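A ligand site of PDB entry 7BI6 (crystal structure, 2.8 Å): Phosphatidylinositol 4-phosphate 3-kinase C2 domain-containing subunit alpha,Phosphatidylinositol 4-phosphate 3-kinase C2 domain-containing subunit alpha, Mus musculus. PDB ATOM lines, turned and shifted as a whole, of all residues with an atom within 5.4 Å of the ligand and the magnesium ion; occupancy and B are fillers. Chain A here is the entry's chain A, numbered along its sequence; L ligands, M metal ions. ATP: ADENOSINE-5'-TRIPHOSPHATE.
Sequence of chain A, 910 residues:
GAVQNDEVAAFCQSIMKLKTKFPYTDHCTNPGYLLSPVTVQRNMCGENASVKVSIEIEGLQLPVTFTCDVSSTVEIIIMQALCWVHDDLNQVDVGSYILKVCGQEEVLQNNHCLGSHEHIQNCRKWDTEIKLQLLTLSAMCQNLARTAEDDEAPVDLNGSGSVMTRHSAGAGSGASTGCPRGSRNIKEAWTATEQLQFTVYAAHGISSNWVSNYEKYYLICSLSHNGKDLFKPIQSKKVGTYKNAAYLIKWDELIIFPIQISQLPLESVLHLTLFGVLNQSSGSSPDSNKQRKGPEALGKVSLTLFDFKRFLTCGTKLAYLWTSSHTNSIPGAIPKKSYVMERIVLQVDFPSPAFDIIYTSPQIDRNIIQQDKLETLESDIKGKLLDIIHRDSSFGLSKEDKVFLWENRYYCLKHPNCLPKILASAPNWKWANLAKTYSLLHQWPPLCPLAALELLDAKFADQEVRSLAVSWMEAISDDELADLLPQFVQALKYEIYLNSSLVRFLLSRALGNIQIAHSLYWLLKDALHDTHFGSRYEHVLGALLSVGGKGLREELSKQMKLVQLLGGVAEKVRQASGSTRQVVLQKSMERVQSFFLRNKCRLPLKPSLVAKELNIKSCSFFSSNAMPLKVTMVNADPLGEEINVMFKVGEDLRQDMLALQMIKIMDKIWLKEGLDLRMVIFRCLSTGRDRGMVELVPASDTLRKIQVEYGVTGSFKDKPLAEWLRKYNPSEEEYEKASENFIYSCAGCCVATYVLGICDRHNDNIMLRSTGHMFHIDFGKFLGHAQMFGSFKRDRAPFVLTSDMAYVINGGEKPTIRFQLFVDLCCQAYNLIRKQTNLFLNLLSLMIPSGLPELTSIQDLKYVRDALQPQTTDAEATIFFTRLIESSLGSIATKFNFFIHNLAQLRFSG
An oxygen (O3G) of the ligand sits at hydrogen-bond distance from the backbone NH (N) of Asn 625, 3.1 Å away. OG of Ser 624 sits at hydrogen-bond distance from O2A of the ligand (2.8 Å). A nitrogen (N6) of the ligand is in hydrogen-bond range of the backbone carbonyl oxygen of Glu 695, 3.0 Å away. N of Val 697 sits at hydrogen-bond distance from N1 of the ligand (2.9 Å). The side-chain amino group of Lys 648 is in salt-bridge range of an oxygen (O1A) of the ligand, 2.7 Å away.
The side-chain amide nitrogen (ND2) of Asn 765 lies within hydrogen-bond range of the side-chain carboxylate (OD2) of Asp 778. The backbone NH (N) of Met 767 sits at hydrogen-bond distance from the backbone carbonyl oxygen (O) of Phe 775, at 2.8 Å. N of Phe 622 sits at hydrogen-bond distance from O of Pro 628 (2.9 Å). O of Asn 765 lies close to N of Ile 777 (3.3 Å). The backbone carbonyl oxygen (O) of Val 697 is in hydrogen-bond range of the side-chain hydroxyl (OG) of Ser 700 (2.7 Å). The backbone NH of Val 694 lies within hydrogen-bond range of the backbone carbonyl oxygen of Met 646, at 2.7 Å. OE1 of Glu 651 lies within salt-bridge range of NZ of Lys 648.
N3 of the ligand sits close to SD of Met 767, at 3.6 Å. O1B of the ligand lies close to OD1 of Asp 778, 3.2 Å away. Phe 622 touches the ligand. Pro 628 touches the ligand (CG to O2A, 3.7 Å). CE of Met 646 touches O4' of the ligand (3.6 Å). Phe 682 touches the ligand (CE1 to N6, 3.5 Å). Leu 696 touches the ligand (CA to N1, 3.6 Å). Thr 702 touches the ligand. Asn 765 touches the ligand. Ile 777 touches the ligand (CG2 to N7, 3.9 Å). Hydrophobic or aromatic side chains within 4 Å of the ligand: Phe 622, Pro 628, Met 646, Phe 682, Leu 696, Val 697, Met 767 and Ile 777. 16 residues have an atom within 4 Å of the ligand: Phe 622, Ser 624, Asn 625, Pro 628, Met 646, Lys 648, Glu 651, Phe 682, Glu 695, Leu 696, Val 697, Thr 702, Asn 765, Met 767, Ile 777 and Asp 778.
Lys 648 touches the magnesium ion. OD1 of Asp 778 touches the magnesium ion, 3.0 Å away. The nearest printed residue that does not touch the magnesium ion is Asp 656 (5.1 Å).
O1B of the ligand binds the magnesium ion (2.4 Å). The magnesium ion has one donor atom within binding distance. Slightly farther from the magnesium ion lies the side-chain carboxylate (OE1) of Glu 651 (2.7 Å).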
ATOM      1  N   PHE A 622      14.622  14.122 -10.676  1.00  0.00           N
ATOM      2  CA  PHE A 622      13.937  13.525 -11.863  1.00  0.00           C
ATOM      3  C   PHE A 622      13.654  14.590 -12.936  1.00  0.00           C
ATOM      4  O   PHE A 622      13.250  14.187 -14.049  1.00  0.00           O
ATOM      5  CB  PHE A 622      12.678  12.770 -11.435  1.00  0.00           C
ATOM      6  CG  PHE A 622      12.910  11.315 -11.137  1.00  0.00           C
ATOM      7  CD1 PHE A 622      13.051  10.411 -12.180  1.00  0.00           C
ATOM      8  CD2 PHE A 622      13.007  10.846  -9.835  1.00  0.00           C
ATOM      9  CE1 PHE A 622      13.278   9.066 -11.921  1.00  0.00           C
ATOM     10  CE2 PHE A 622      13.224   9.504  -9.575  1.00  0.00           C
ATOM     11  CZ  PHE A 622      13.357   8.611 -10.621  1.00  0.00           C
ATOM     12  N   SER A 624      11.361  17.165 -13.409  1.00  0.00           N
ATOM     13  CA  SER A 624       9.935  17.338 -13.807  1.00  0.00           C
ATOM     14  C   SER A 624       9.254  18.312 -12.838  1.00  0.00           C
ATOM     15  O   SER A 624       9.971  18.978 -12.071  1.00  0.00           O
ATOM     16  CB  SER A 624       9.234  16.004 -13.866  1.00  0.00           C
ATOM     17  OG  SER A 624       9.091  15.441 -12.573  1.00  0.00           O
ATOM     18  N   ASN A 625       7.915  18.402 -12.881  1.00  0.00           N
ATOM     19  CA  ASN A 625       7.113  19.234 -11.946  1.00  0.00           C
ATOM     20  C   ASN A 625       7.279  18.686 -10.525  1.00  0.00           C
ATOM     21  O   ASN A 625       7.094  17.471 -10.343  1.00  0.00           O
ATOM     22  CB  ASN A 625       5.630  19.278 -12.353  1.00  0.00           C
ATOM     23  CG  ASN A 625       4.841  20.349 -11.631  1.00  0.00           C
ATOM     24  OD1 ASN A 625       5.410  21.264 -11.042  1.00  0.00           O
ATOM     25  ND2 ASN A 625       3.524  20.251 -11.679  1.00  0.00           N
ATOM     26  N   ALA A 626       7.657  19.564  -9.580  1.00  0.00           N
ATOM     27  CA  ALA A 626       7.906  19.278  -8.142  1.00  0.00           C
ATOM     28  C   ALA A 626       9.382  18.898  -7.911  1.00  0.00           C
ATOM     29  O   ALA A 626       9.795  18.893  -6.741  1.00  0.00           O
ATOM     30  CB  ALA A 626       6.981  18.203  -7.644  1.00  0.00           C
ATOM     31  N   PRO A 628      11.119  15.836  -8.152  1.00  0.00           N
ATOM     32  CA  PRO A 628      11.242  14.706  -7.232  1.00  0.00           C
ATOM     33  C   PRO A 628      12.695  14.207  -7.103  1.00  0.00           C
ATOM     34  O   PRO A 628      13.419  14.279  -8.083  1.00  0.00           O
ATOM     35  CB  PRO A 628      10.380  13.598  -7.864  1.00  0.00           C
ATOM     36  CG  PRO A 628       9.468  14.329  -8.837  1.00  0.00           C
ATOM     37  CD  PRO A 628      10.278  15.505  -9.323  1.00  0.00           C
ATOM     38  N   MET A 646      11.895   7.070  -4.647  1.00  0.00           N
ATOM     39  CA  MET A 646      11.644   8.498  -4.982  1.00  0.00           C
ATOM     40  C   MET A 646      11.001   9.176  -3.783  1.00  0.00           C
ATOM     41  O   MET A 646      10.079   8.568  -3.205  1.00  0.00           O
ATOM     42  CB  MET A 646      10.722   8.614  -6.204  1.00  0.00           C
ATOM     43  CG  MET A 646      10.267  10.043  -6.489  1.00  0.00           C
ATOM     44  SD  MET A 646       8.813  10.110  -7.564  1.00  0.00           S
ATOM     45  CE  MET A 646       9.535   9.669  -9.144  1.00  0.00           C
ATOM     46  N   LYS A 648       8.991  12.731  -3.136  1.00  0.00           N
ATOM     47  CA  LYS A 648       8.302  13.875  -3.790  1.00  0.00           C
ATOM     48  C   LYS A 648       7.742  14.805  -2.714  1.00  0.00           C
ATOM     49  O   LYS A 648       7.334  14.303  -1.641  1.00  0.00           O
ATOM     50  CB  LYS A 648       7.192  13.362  -4.714  1.00  0.00           C
ATOM     51  CG  LYS A 648       6.636  14.381  -5.694  1.00  0.00           C
ATOM     52  CD  LYS A 648       5.308  13.994  -6.289  1.00  0.00           C
ATOM     53  CE  LYS A 648       5.406  12.911  -7.352  1.00  0.00           C
ATOM     54  NZ  LYS A 648       5.720  13.491  -8.678  1.00  0.00           N
ATOM     55  N   GLU A 651       2.863  17.592  -3.790  1.00  0.00           N
ATOM     56  CA  GLU A 651       1.659  16.864  -4.262  1.00  0.00           C
ATOM     57  C   GLU A 651       1.108  15.986  -3.131  1.00  0.00           C
ATOM     58  O   GLU A 651       1.915  15.387  -2.393  1.00  0.00           O
ATOM     59  CB  GLU A 651       1.986  16.007  -5.489  1.00  0.00           C
ATOM     60  CG  GLU A 651       2.557  16.805  -6.651  1.00  0.00           C
ATOM     61  CD  GLU A 651       2.676  16.045  -7.966  1.00  0.00           C
ATOM     62  OE1 GLU A 651       2.240  14.880  -8.016  1.00  0.00           O
ATOM     63  OE2 GLU A 651       3.205  16.631  -8.934  1.00  0.00           O
ATOM     64  N   ASP A 656      -3.114   9.142  -5.032  1.00  0.00           N
ATOM     65  CA  ASP A 656      -2.193   8.192  -5.696  1.00  0.00           C
ATOM     66  C   ASP A 656      -2.233   6.862  -4.934  1.00  0.00           C
ATOM     67  O   ASP A 656      -2.305   5.807  -5.606  1.00  0.00           O
ATOM     68  CB  ASP A 656      -0.771   8.755  -5.794  1.00  0.00           C
ATOM     69  CG  ASP A 656      -0.598   9.850  -6.826  1.00  0.00           C
ATOM     70  OD1 ASP A 656      -1.573  10.594  -7.060  1.00  0.00           O
ATOM     71  OD2 ASP A 656       0.510   9.961  -7.383  1.00  0.00           O
ATOM     72  N   PHE A 682       3.266  -1.398  -7.407  1.00  0.00           N
ATOM     73  CA  PHE A 682       4.334  -0.616  -6.731  1.00  0.00           C
ATOM     74  C   PHE A 682       3.735   0.193  -5.571  1.00  0.00           C
ATOM     75  O   PHE A 682       2.538   0.566  -5.642  1.00  0.00           O
ATOM     76  CB  PHE A 682       5.110   0.247  -7.735  1.00  0.00           C
ATOM     77  CG  PHE A 682       4.403   1.470  -8.264  1.00  0.00           C
ATOM     78  CD1 PHE A 682       4.367   2.640  -7.530  1.00  0.00           C
ATOM     79  CD2 PHE A 682       3.809   1.455  -9.517  1.00  0.00           C
ATOM     80  CE1 PHE A 682       3.736   3.774  -8.029  1.00  0.00           C
ATOM     81  CE2 PHE A 682       3.178   2.589 -10.016  1.00  0.00           C
ATOM     82  CZ  PHE A 682       3.141   3.744  -9.270  1.00  0.00           C
ATOM     83  N   VAL A 694       7.826   7.116  -3.067  1.00  0.00           N
ATOM     84  CA  VAL A 694       7.194   6.214  -4.080  1.00  0.00           C
ATOM     85  C   VAL A 694       8.222   5.159  -4.491  1.00  0.00           C
ATOM     86  O   VAL A 694       9.399   5.524  -4.693  1.00  0.00           O
ATOM     87  CB  VAL A 694       6.695   7.007  -5.297  1.00  0.00           C
ATOM     88  CG1 VAL A 694       5.712   6.215  -6.132  1.00  0.00           C
ATOM     89  CG2 VAL A 694       6.097   8.355  -4.908  1.00  0.00           C
ATOM     90  N   GLU A 695       7.797   3.890  -4.618  1.00  0.00           N
ATOM     91  CA  GLU A 695       8.637   2.776  -5.131  1.00  0.00           C
ATOM     92  C   GLU A 695       8.977   3.056  -6.598  1.00  0.00           C
ATOM     93  O   GLU A 695       8.053   3.339  -7.376  1.00  0.00           O
ATOM     94  CB  GLU A 695       7.893   1.434  -5.014  1.00  0.00           C
ATOM     95  CG  GLU A 695       8.708   0.242  -5.482  1.00  0.00           C
ATOM     96  CD  GLU A 695       8.017  -1.103  -5.362  1.00  0.00           C
ATOM     97  OE1 GLU A 695       7.054  -1.217  -4.580  1.00  0.00           O
ATOM     98  OE2 GLU A 695       8.442  -2.047  -6.061  1.00  0.00           O
ATOM     99  N   LEU A 696      10.268   2.994  -6.943  1.00  0.00           N
ATOM    100  CA  LEU A 696      10.768   3.174  -8.334  1.00  0.00           C
ATOM    101  C   LEU A 696      10.879   1.790  -9.001  1.00  0.00           C
ATOM    102  O   LEU A 696      11.756   1.006  -8.592  1.00  0.00           O
ATOM    103  CB  LEU A 696      12.131   3.883  -8.309  1.00  0.00           C
ATOM    104  CG  LEU A 696      12.080   5.370  -7.953  1.00  0.00           C
ATOM    105  CD1 LEU A 696      13.480   5.915  -7.742  1.00  0.00           C
ATOM    106  CD2 LEU A 696      11.354   6.157  -9.036  1.00  0.00           C
ATOM    107  N   VAL A 697      10.003   1.521  -9.972  1.00  0.00           N
ATOM    108  CA  VAL A 697      10.001   0.273 -10.791  1.00  0.00           C
ATOM    109  C   VAL A 697      11.255   0.283 -11.658  1.00  0.00           C
ATOM    110  O   VAL A 697      11.461   1.209 -12.431  1.00  0.00           O
ATOM    111  CB  VAL A 697       8.715   0.149 -11.646  1.00  0.00           C
ATOM    112  CG1 VAL A 697       8.702  -1.133 -12.461  1.00  0.00           C
ATOM    113  CG2 VAL A 697       7.453   0.264 -10.802  1.00  0.00           C
ATOM    114  N   SER A 700      12.386   0.550 -16.479  1.00  0.00           N
ATOM    115  CA  SER A 700      11.082   1.000 -17.013  1.00  0.00           C
ATOM    116  C   SER A 700      11.157   2.483 -17.421  1.00  0.00           C
ATOM    117  O   SER A 700      11.742   3.272 -16.651  1.00  0.00           O
ATOM    118  CB  SER A 700       9.986   0.771 -16.009  1.00  0.00           C
ATOM    119  OG  SER A 700      10.236   1.492 -14.813  1.00  0.00           O
ATOM    120  N   THR A 702       8.708   5.765 -19.723  1.00  0.00           N
ATOM    121  CA  THR A 702       7.369   6.221 -20.190  1.00  0.00           C
ATOM    122  C   THR A 702       7.232   5.906 -21.681  1.00  0.00           C
ATOM    123  O   THR A 702       8.278   5.832 -22.364  1.00  0.00           O
ATOM    124  CB  THR A 702       7.149   7.723 -19.920  1.00  0.00           C
ATOM    125  OG1 THR A 702       8.037   8.464 -20.756  1.00  0.00           O
ATOM    126  CG2 THR A 702       7.374   8.108 -18.473  1.00  0.00           C
ATOM    127  N   ASP A 764       2.943  10.070 -21.390  1.00  0.00           N
ATOM    128  CA  ASP A 764       3.776  10.387 -20.190  1.00  0.00           C
ATOM    129  C   ASP A 764       3.257   9.626 -18.960  1.00  0.00           C
ATOM    130  O   ASP A 764       4.086   9.215 -18.131  1.00  0.00           O
ATOM    131  CB  ASP A 764       3.802  11.898 -19.905  1.00  0.00           C
ATOM    132  CG  ASP A 764       5.116  12.580 -20.239  1.00  0.00           C
ATOM    133  OD1 ASP A 764       6.159  11.882 -20.304  1.00  0.00           O
ATOM    134  OD2 ASP A 764       5.100  13.814 -20.427  1.00  0.00           O
ATOM    135  N   ASN A 765       1.933   9.448 -18.851  1.00  0.00           N
ATOM    136  CA  ASN A 765       1.251   8.927 -17.636  1.00  0.00           C
ATOM    137  C   ASN A 765       1.279   7.401 -17.614  1.00  0.00           C
ATOM    138  O   ASN A 765       1.225   6.830 -16.509  1.00  0.00           O
ATOM    139  CB  ASN A 765      -0.171   9.492 -17.520  1.00  0.00           C
ATOM    140  CG  ASN A 765      -0.189  10.957 -17.138  1.00  0.00           C
ATOM    141  OD1 ASN A 765       0.809  11.662 -17.300  1.00  0.00           O
ATOM    142  ND2 ASN A 765      -1.323  11.433 -16.643  1.00  0.00           N
ATOM    143  N   MET A 767       3.517   3.951 -18.226  1.00  0.00           N
ATOM    144  CA  MET A 767       4.927   3.489 -18.184  1.00  0.00           C
ATOM    145  C   MET A 767       4.995   2.018 -18.615  1.00  0.00           C
ATOM    146  O   MET A 767       3.958   1.319 -18.531  1.00  0.00           O
ATOM    147  CB  MET A 767       5.525   3.633 -16.788  1.00  0.00           C
ATOM    148  CG  MET A 767       6.145   4.994 -16.533  1.00  0.00           C
ATOM    149  SD  MET A 767       7.329   5.000 -15.171  1.00  0.00           S
ATOM    150  CE  MET A 767       8.675   4.060 -15.886  1.00  0.00           C
ATOM    151  N   PHE A 775       2.012  -0.286 -16.896  1.00  0.00           N
ATOM    152  CA  PHE A 775       1.456   0.187 -15.601  1.00  0.00           C
ATOM    153  C   PHE A 775       1.305   1.725 -15.611  1.00  0.00           C
ATOM    154  O   PHE A 775       2.061   2.405 -16.333  1.00  0.00           O
ATOM    155  CB  PHE A 775       2.330  -0.283 -14.440  1.00  0.00           C
ATOM    156  CG  PHE A 775       3.749   0.220 -14.437  1.00  0.00           C
ATOM    157  CD1 PHE A 775       4.721  -0.376 -15.231  1.00  0.00           C
ATOM    158  CD2 PHE A 775       4.132   1.271 -13.612  1.00  0.00           C
ATOM    159  CE1 PHE A 775       6.029   0.075 -15.213  1.00  0.00           C
ATOM    160  CE2 PHE A 775       5.436   1.724 -13.607  1.00  0.00           C
ATOM    161  CZ  PHE A 775       6.387   1.129 -14.404  1.00  0.00           C
ATOM    162  N   ILE A 777       1.368   5.481 -13.529  1.00  0.00           N
ATOM    163  CA  ILE A 777       2.218   6.146 -12.504  1.00  0.00           C
ATOM    164  C   ILE A 777       1.510   7.390 -11.940  1.00  0.00           C
ATOM    165  O   ILE A 777       1.529   7.550 -10.705  1.00  0.00           O
ATOM    166  CB  ILE A 777       3.619   6.476 -13.051  1.00  0.00           C
ATOM    167  CG1 ILE A 777       3.583   7.248 -14.383  1.00  0.00           C
ATOM    168  CG2 ILE A 777       4.455   5.209 -13.178  1.00  0.00           C
ATOM    169  CD1 ILE A 777       4.806   8.105 -14.627  1.00  0.00           C
ATOM    170  N   ASP A 778       0.935   8.225 -12.799  1.00  0.00           N
ATOM    171  CA  ASP A 778       0.230   9.483 -12.408  1.00  0.00           C
ATOM    172  C   ASP A 778      -1.254   9.165 -12.193  1.00  0.00           C
ATOM    173  O   ASP A 778      -1.838   8.490 -13.063  1.00  0.00           O
ATOM    174  CB  ASP A 778       0.427  10.570 -13.461  1.00  0.00           C
ATOM    175  CG  ASP A 778      -0.054  11.941 -13.026  1.00  0.00           C
ATOM    176  OD1 ASP A 778       0.383  12.410 -11.954  1.00  0.00           O
ATOM    177  OD2 ASP A 778      -0.871  12.542 -13.761  1.00  0.00           O
HETATM  178  PG  ATP L   1       4.657  15.970 -13.669  1.00  0.00           P
HETATM  179  O1G ATP L   1       4.936  15.785 -12.200  1.00  0.00           O
HETATM  180  O2G ATP L   1       3.276  16.509 -13.946  1.00  0.00           O
HETATM  181  O3G ATP L   1       5.741  16.764 -14.361  1.00  0.00           O
HETATM  182  PB  ATP L   1       4.308  13.052 -13.760  1.00  0.00           P
HETATM  183  O1B ATP L   1       3.435  13.232 -12.555  1.00  0.00           O
HETATM  184  O2B ATP L   1       3.837  12.209 -14.899  1.00  0.00           O
HETATM  185  O3B ATP L   1       4.698  14.497 -14.328  1.00  0.00           O
HETATM  186  PA  ATP L   1       6.462  12.477 -11.852  1.00  0.00           P
HETATM  187  O1A ATP L   1       5.520  11.901 -10.855  1.00  0.00           O
HETATM  188  O2A ATP L   1       7.061  13.821 -11.573  1.00  0.00           O
HETATM  189  O3A ATP L   1       5.743  12.523 -13.288  1.00  0.00           O
HETATM  190  O5' ATP L   1       7.647  11.431 -12.133  1.00  0.00           O
HETATM  191  C5' ATP L   1       8.760  11.842 -12.973  1.00  0.00           C
HETATM  192  C4' ATP L   1       9.335  10.634 -13.672  1.00  0.00           C
HETATM  193  O4' ATP L   1       9.703   9.637 -12.693  1.00  0.00           O
HETATM  194  C3' ATP L   1       8.385   9.901 -14.621  1.00  0.00           C
HETATM  195  O3' ATP L   1       8.367  10.498 -15.911  1.00  0.00           O
HETATM  196  C2' ATP L   1       9.003   8.493 -14.651  1.00  0.00           C
HETATM  197  O2' ATP L   1      10.051   8.394 -15.587  1.00  0.00           O
HETATM  198  C1' ATP L   1       9.532   8.343 -13.228  1.00  0.00           C
HETATM  199  N9  ATP L   1       8.634   7.594 -12.341  1.00  0.00           N
HETATM  200  C8  ATP L   1       7.532   8.058 -11.665  1.00  0.00           C
HETATM  201  N7  ATP L   1       6.951   7.129 -10.953  1.00  0.00           N
HETATM  202  C5  ATP L   1       7.709   5.987 -11.161  1.00  0.00           C
HETATM  203  C6  ATP L   1       7.609   4.665 -10.684  1.00  0.00           C
HETATM  204  N6  ATP L   1       6.668   4.252  -9.852  1.00  0.00           N
HETATM  205  N1  ATP L   1       8.551   3.776 -11.095  1.00  0.00           N
HETATM  206  C2  ATP L   1       9.504   4.200 -11.943  1.00  0.00           C
HETATM  207  N3  ATP L   1       9.700   5.416 -12.456  1.00  0.00           N
HETATM  208  C4  ATP L   1       8.754   6.274 -12.020  1.00  0.00           C
HETATM  209 MG    MG M   1       2.557  13.567 -10.316  1.00  0.00          MG
